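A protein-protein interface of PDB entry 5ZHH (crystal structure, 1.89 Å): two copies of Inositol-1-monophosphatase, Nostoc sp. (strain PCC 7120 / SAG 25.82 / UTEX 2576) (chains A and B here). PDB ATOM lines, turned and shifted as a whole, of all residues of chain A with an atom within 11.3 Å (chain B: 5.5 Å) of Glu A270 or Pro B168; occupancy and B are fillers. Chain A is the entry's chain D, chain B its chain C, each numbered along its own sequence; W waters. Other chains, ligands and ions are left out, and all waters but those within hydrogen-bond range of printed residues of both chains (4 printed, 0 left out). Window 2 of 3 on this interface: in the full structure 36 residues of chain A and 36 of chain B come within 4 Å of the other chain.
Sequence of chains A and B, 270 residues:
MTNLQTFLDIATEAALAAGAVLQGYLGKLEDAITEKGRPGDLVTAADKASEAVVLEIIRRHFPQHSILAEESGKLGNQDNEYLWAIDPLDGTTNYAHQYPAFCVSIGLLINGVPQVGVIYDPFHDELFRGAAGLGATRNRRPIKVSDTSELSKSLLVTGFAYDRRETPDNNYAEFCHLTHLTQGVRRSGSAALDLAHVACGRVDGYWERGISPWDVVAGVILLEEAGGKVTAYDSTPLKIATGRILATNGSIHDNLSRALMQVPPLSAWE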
ATOM      1  N   CYS A 176       0.737   7.482  -0.086  1.00  0.00           N
ATOM      2  CA  CYS A 176       1.060   6.180  -0.605  1.00  0.00           C
ATOM      3  C   CYS A 176       0.855   6.112  -2.101  1.00  0.00           C
ATOM      4  O   CYS A 176       1.658   5.661  -2.776  1.00  0.00           O
ATOM      5  CB  CYS A 176       0.240   5.124   0.077  1.00  0.00           C
ATOM      6  SG  CYS A 176       0.507   5.011   1.841  1.00  0.00           S
ATOM      7  N   HIS A 180       3.979   5.651  -4.909  1.00  0.00           N
ATOM      8  CA  HIS A 180       3.995   4.623  -5.903  1.00  0.00           C
ATOM      9  C   HIS A 180       4.117   5.116  -7.348  1.00  0.00           C
ATOM     10  O   HIS A 180       4.639   4.465  -8.141  1.00  0.00           O
ATOM     11  CB  HIS A 180       2.724   3.845  -5.826  1.00  0.00           C
ATOM     12  CG  HIS A 180       2.917   2.462  -5.339  1.00  0.00           C
ATOM     13  ND1 HIS A 180       2.304   1.390  -5.919  1.00  0.00           N
ATOM     14  CD2 HIS A 180       3.654   1.976  -4.324  1.00  0.00           C
ATOM     15  CE1 HIS A 180       2.632   0.305  -5.271  1.00  0.00           C
ATOM     16  NE2 HIS A 180       3.458   0.633  -4.302  1.00  0.00           N
ATOM     17  N   PRO A 264      -6.890   5.891  -4.407  1.00  0.00           N
ATOM     18  CA  PRO A 264      -7.529   4.740  -3.755  1.00  0.00           C
ATOM     19  C   PRO A 264      -7.431   4.868  -2.247  1.00  0.00           C
ATOM     20  O   PRO A 264      -6.427   5.380  -1.723  1.00  0.00           O
ATOM     21  CB  PRO A 264      -6.705   3.541  -4.260  1.00  0.00           C
ATOM     22  CG  PRO A 264      -5.932   4.053  -5.439  1.00  0.00           C
ATOM     23  CD  PRO A 264      -5.654   5.503  -5.104  1.00  0.00           C
ATOM     24  N   PRO A 265      -8.445   4.426  -1.508  1.00  0.00           N
ATOM     25  CA  PRO A 265      -8.349   4.463  -0.046  1.00  0.00           C
ATOM     26  C   PRO A 265      -7.323   3.456   0.449  1.00  0.00           C
ATOM     27  O   PRO A 265      -6.962   2.502  -0.243  1.00  0.00           O
ATOM     28  CB  PRO A 265      -9.762   4.093   0.425  1.00  0.00           C
ATOM     29  CG  PRO A 265     -10.351   3.292  -0.715  1.00  0.00           C
ATOM     30  CD  PRO A 265      -9.676   3.762  -1.987  1.00  0.00           C
ATOM     31  N   LEU A 266      -6.862   3.677   1.684  1.00  0.00           N
ATOM     32  CA  LEU A 266      -5.885   2.777   2.293  1.00  0.00           C
ATOM     33  C   LEU A 266      -6.420   1.354   2.354  1.00  0.00           C
ATOM     34  O   LEU A 266      -5.671   0.383   2.179  1.00  0.00           O
ATOM     35  CB  LEU A 266      -5.547   3.268   3.701  1.00  0.00           C
ATOM     36  CG  LEU A 266      -4.658   4.515   3.796  1.00  0.00           C
ATOM     37  CD1 LEU A 266      -4.436   4.875   5.257  1.00  0.00           C
ATOM     38  CD2 LEU A 266      -3.335   4.268   3.114  1.00  0.00           C
ATOM     39  N   SER A 267      -7.721   1.222   2.604  1.00  0.00           N
ATOM     40  CA  SER A 267      -8.380  -0.071   2.683  1.00  0.00           C
ATOM     41  C   SER A 267      -8.274  -0.875   1.391  1.00  0.00           C
ATOM     42  O   SER A 267      -8.507  -2.091   1.412  1.00  0.00           O
ATOM     43  CB  SER A 267      -9.838   0.148   3.080  1.00  0.00           C
ATOM     44  OG  SER A 267     -10.514   0.937   2.118  1.00  0.00           O
ATOM     45  N   ALA A 268      -7.959  -0.227   0.264  1.00  0.00           N
ATOM     46  CA  ALA A 268      -7.808  -0.935  -1.003  1.00  0.00           C
ATOM     47  C   ALA A 268      -6.439  -1.586  -1.172  1.00  0.00           C
ATOM     48  O   ALA A 268      -6.255  -2.358  -2.117  1.00  0.00           O
ATOM     49  CB  ALA A 268      -8.060   0.017  -2.172  1.00  0.00           C
ATOM     50  N   TRP A 269      -5.484  -1.293  -0.294  1.00  0.00           N
ATOM     51  CA  TRP A 269      -4.161  -1.898  -0.310  1.00  0.00           C
ATOM     52  C   TRP A 269      -4.165  -3.209   0.471  1.00  0.00           C
ATOM     53  O   TRP A 269      -5.062  -3.482   1.268  1.00  0.00           O
ATOM     54  CB  TRP A 269      -3.141  -0.937   0.302  1.00  0.00           C
ATOM     55  CG  TRP A 269      -2.935   0.334  -0.464  1.00  0.00           C
ATOM     56  CD1 TRP A 269      -3.792   1.399  -0.532  1.00  0.00           C
ATOM     57  CD2 TRP A 269      -1.770   0.712  -1.212  1.00  0.00           C
ATOM     58  NE1 TRP A 269      -3.241   2.404  -1.301  1.00  0.00           N
ATOM     59  CE2 TRP A 269      -2.002   2.003  -1.731  1.00  0.00           C
ATOM     60  CE3 TRP A 269      -0.557   0.078  -1.501  1.00  0.00           C
ATOM     61  CZ2 TRP A 269      -1.063   2.677  -2.513  1.00  0.00           C
ATOM     62  CZ3 TRP A 269       0.376   0.750  -2.288  1.00  0.00           C
ATOM     63  CH2 TRP A 269       0.112   2.029  -2.788  1.00  0.00           C
ATOM     64  N   GLU A 270      -3.145  -4.025   0.239  1.00  0.00           N
ATOM     65  CA  GLU A 270      -2.913  -5.166   1.121  1.00  0.00           C
ATOM     66  C   GLU A 270      -2.276  -4.679   2.418  1.00  0.00           C
ATOM     67  O   GLU A 270      -1.189  -4.092   2.399  1.00  0.00           O
ATOM     68  CB  GLU A 270      -2.011  -6.216   0.475  1.00  0.00           C
ATOM     69  CG  GLU A 270      -2.297  -6.530  -0.978  1.00  0.00           C
ATOM     70  CD  GLU A 270      -1.349  -7.600  -1.516  1.00  0.00           C
ATOM     71  OE1 GLU A 270      -0.841  -7.442  -2.660  1.00  0.00           O
ATOM     72  OE2 GLU A 270      -1.091  -8.592  -0.778  1.00  0.00           O
ATOM     73  N   GLU B 166       6.662  -3.694  -6.037  1.00  0.00           N
ATOM     74  CA  GLU B 166       6.700  -5.115  -6.353  1.00  0.00           C
ATOM     75  C   GLU B 166       6.419  -6.026  -5.174  1.00  0.00           C
ATOM     76  O   GLU B 166       6.277  -7.243  -5.376  1.00  0.00           O
ATOM     77  CB  GLU B 166       8.067  -5.429  -6.965  1.00  0.00           C
ATOM     78  CG  GLU B 166       8.051  -4.961  -8.382  1.00  0.00           C
ATOM     79  CD  GLU B 166       8.696  -3.615  -8.539  1.00  0.00           C
ATOM     80  OE1 GLU B 166       9.047  -2.999  -7.493  1.00  0.00           O
ATOM     81  OE2 GLU B 166       8.855  -3.178  -9.699  1.00  0.00           O
ATOM     82  N   THR B 167       6.427  -5.499  -3.954  1.00  0.00           N
ATOM     83  CA  THR B 167       6.159  -6.266  -2.757  1.00  0.00           C
ATOM     84  C   THR B 167       5.103  -5.550  -1.936  1.00  0.00           C
ATOM     85  O   THR B 167       5.034  -4.316  -1.948  1.00  0.00           O
ATOM     86  CB  THR B 167       7.445  -6.432  -1.935  1.00  0.00           C
ATOM     87  OG1 THR B 167       7.134  -6.946  -0.649  1.00  0.00           O
ATOM     88  CG2 THR B 167       8.182  -5.092  -1.816  1.00  0.00           C
ATOM     89  N   PRO B 168       4.264  -6.296  -1.220  1.00  0.00           N
ATOM     90  CA  PRO B 168       3.343  -5.650  -0.278  1.00  0.00           C
ATOM     91  C   PRO B 168       4.061  -5.025   0.901  1.00  0.00           C
ATOM     92  O   PRO B 168       3.496  -4.141   1.561  1.00  0.00           O
ATOM     93  CB  PRO B 168       2.424  -6.802   0.171  1.00  0.00           C
ATOM     94  CG  PRO B 168       2.633  -7.899  -0.832  1.00  0.00           C
ATOM     95  CD  PRO B 168       4.049  -7.750  -1.307  1.00  0.00           C
ATOM     96  N   ASP B 169       5.279  -5.478   1.198  1.00  0.00           N
ATOM     97  CA  ASP B 169       6.103  -4.893   2.253  1.00  0.00           C
ATOM     98  C   ASP B 169       6.817  -3.656   1.699  1.00  0.00           C
ATOM     99  O   ASP B 169       8.010  -3.657   1.385  1.00  0.00           O
ATOM    100  CB  ASP B 169       7.084  -5.924   2.794  1.00  0.00           C
ATOM    101  CG  ASP B 169       7.800  -5.446   4.044  1.00  0.00           C
ATOM    102  OD1 ASP B 169       7.307  -4.486   4.680  1.00  0.00           O
ATOM    103  OD2 ASP B 169       8.850  -6.035   4.386  1.00  0.00           O
ATOM    104  N   ASN B 170       6.040  -2.589   1.539  1.00  0.00           N
ATOM    105  CA  ASN B 170       6.511  -1.358   0.922  1.00  0.00           C
ATOM    106  C   ASN B 170       6.868  -0.264   1.924  1.00  0.00           C
ATOM    107  O   ASN B 170       7.309   0.813   1.503  1.00  0.00           O
ATOM    108  CB  ASN B 170       5.443  -0.838  -0.037  1.00  0.00           C
ATOM    109  CG  ASN B 170       4.063  -0.876   0.579  1.00  0.00           C
ATOM    110  OD1 ASN B 170       3.901  -0.621   1.773  1.00  0.00           O
ATOM    111  ND2 ASN B 170       3.060  -1.233  -0.221  1.00  0.00           N
ATOM    112  N   ASN B 171       6.699  -0.514   3.228  1.00  0.00           N
ATOM    113  CA  ASN B 171       6.984   0.389   4.350  1.00  0.00           C
ATOM    114  C   ASN B 171       5.889   1.435   4.546  1.00  0.00           C
ATOM    115  O   ASN B 171       6.026   2.291   5.434  1.00  0.00           O
ATOM    116  CB  ASN B 171       8.338   1.110   4.214  1.00  0.00           C
ATOM    117  CG  ASN B 171       8.860   1.630   5.534  1.00  0.00           C
ATOM    118  OD1 ASN B 171       8.740   0.966   6.562  1.00  0.00           O
ATOM    119  ND2 ASN B 171       9.459   2.822   5.512  1.00  0.00           N
ATOM    120  N   PRO B 265      -1.662  -3.575   9.107  1.00  0.00           N
ATOM    121  CA  PRO B 265      -1.560  -3.443   7.649  1.00  0.00           C
ATOM    122  C   PRO B 265      -2.391  -2.278   7.144  1.00  0.00           C
ATOM    123  O   PRO B 265      -3.298  -1.787   7.820  1.00  0.00           O
ATOM    124  CB  PRO B 265      -2.116  -4.775   7.128  1.00  0.00           C
ATOM    125  CG  PRO B 265      -3.040  -5.252   8.218  1.00  0.00           C
ATOM    126  CD  PRO B 265      -2.528  -4.704   9.518  1.00  0.00           C
ATOM    127  N   LEU B 266      -2.071  -1.840   5.921  1.00  0.00           N
ATOM    128  CA  LEU B 266      -2.808  -0.734   5.312  1.00  0.00           C
ATOM    129  C   LEU B 266      -4.287  -1.061   5.189  1.00  0.00           C
ATOM    130  O   LEU B 266      -5.145  -0.182   5.342  1.00  0.00           O
ATOM    131  CB  LEU B 266      -2.237  -0.415   3.930  1.00  0.00           C
ATOM    132  CG  LEU B 266      -0.908   0.327   3.884  1.00  0.00           C
ATOM    133  CD1 LEU B 266      -0.509   0.537   2.431  1.00  0.00           C
ATOM    134  CD2 LEU B 266      -1.030   1.649   4.619  1.00  0.00           C
ATOM    135  N   SER B 267      -4.600  -2.323   4.894  1.00  0.00           N
ATOM    136  CA  SER B 267      -5.979  -2.770   4.748  1.00  0.00           C
ATOM    137  C   SER B 267      -6.811  -2.569   6.012  1.00  0.00           C
ATOM    138  O   SER B 267      -8.044  -2.567   5.930  1.00  0.00           O
ATOM    139  CB  SER B 267      -5.968  -4.232   4.305  1.00  0.00           C
ATOM    140  OG  SER B 267      -5.317  -5.042   5.265  1.00  0.00           O
HETATM  141  O   HOH W   1       0.892  -3.034   0.682  1.00  0.00           O
HETATM  142  O   HOH W   2       3.288  -2.224  -2.991  1.00  0.00           O
HETATM  143  O   HOH W   3      -9.732  -3.587   3.858  1.00  0.00           O
HETATM  144  O   HOH W   4       0.251  -2.989   4.576  1.00  0.00           O
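O of Leu A266 lies close to O of Leu B266 (3.3 Å).
Water W4 bridges the backbone carbonyl oxygen (O) of Glu A270 (2.8 Å) and the backbone NH (N) of Leu B266 (2.9 Å). Water W3 bridges O of Ser B267 (2.9 Å) and O of Ser A267 (3.1 Å). Water W1 lies within hydrogen-bond range of O of Glu A270 (2.9 Å), ND2 of Asn B170 (3.0 Å) and O of Pro B168 (3.0 Å). Water W2 lies within hydrogen-bond range of the backbone carbonyl oxygen (O) of Thr B167 (2.9 Å), the side-chain amide nitrogen (ND2) of Asn B170 (3.0 Å) and a ring nitrogen (NE2) of His A180 (3.1 Å).
Leu B266 touches its own counterpart, Leu A266. Leu A266 touches Ser B267, but with the chains exchanged Ser A267 does not touch Leu B266 (4.01 Å). 3 positions are printed for both chains. Of the 6 pairs that touch across the chains among the printed residues, 1 has its exchanged pair printed and touching as well.
O of Pro B168 sits at hydrogen-bond distance from ND2 of Asn B170, at 3.4 Å.
Of chain B, only Pro B168 comes within 4 Å of Glu A270. Of chain A, only Glu A270 comes within 4 Å of Pro B168. No residue of chain A comes within 4 Å of Thr B167. No residue of chain A comes within 4 Å of Asp B169. Of chain A, only Trp A269 (3.9 Å) comes within 4 Å of Asn B170. Of the printed residues of chain B, Trp A269 touches Asn B170, Leu B266 and Ser B267. Printed residues of chain A within 4 Å of Leu B266: Leu A266 (3.3 Å) and Trp A269 (3.7 Å). The nearest printed residue of chain B that does not touch Glu A270 is Leu B266 (4.1 Å). The nearest printed residue of chain B that does not touch Trp A269 is Pro B265 (6.6 Å).
Among the printed residues, merely in contact across the chains: Trp A269 with Ser B267, Trp A269 with Leu B266, Glu A270 with Pro B168, Trp A269 with Asn B170 and Leu A266 with Ser B267.
Of the 9 printed residues of chain A, 3 touch a printed residue of chain B. Hydrophobic or aromatic side chains of chain A within 4 Å of the printed part of chain B: Leu A266 and Trp A269. Among the printed residues, 6 pairs touch across the chains. Among the printed residues, no Asp or Glu carboxylate lies within 4 Å of a Lys or Arg side-chain nitrogen of the other chain.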
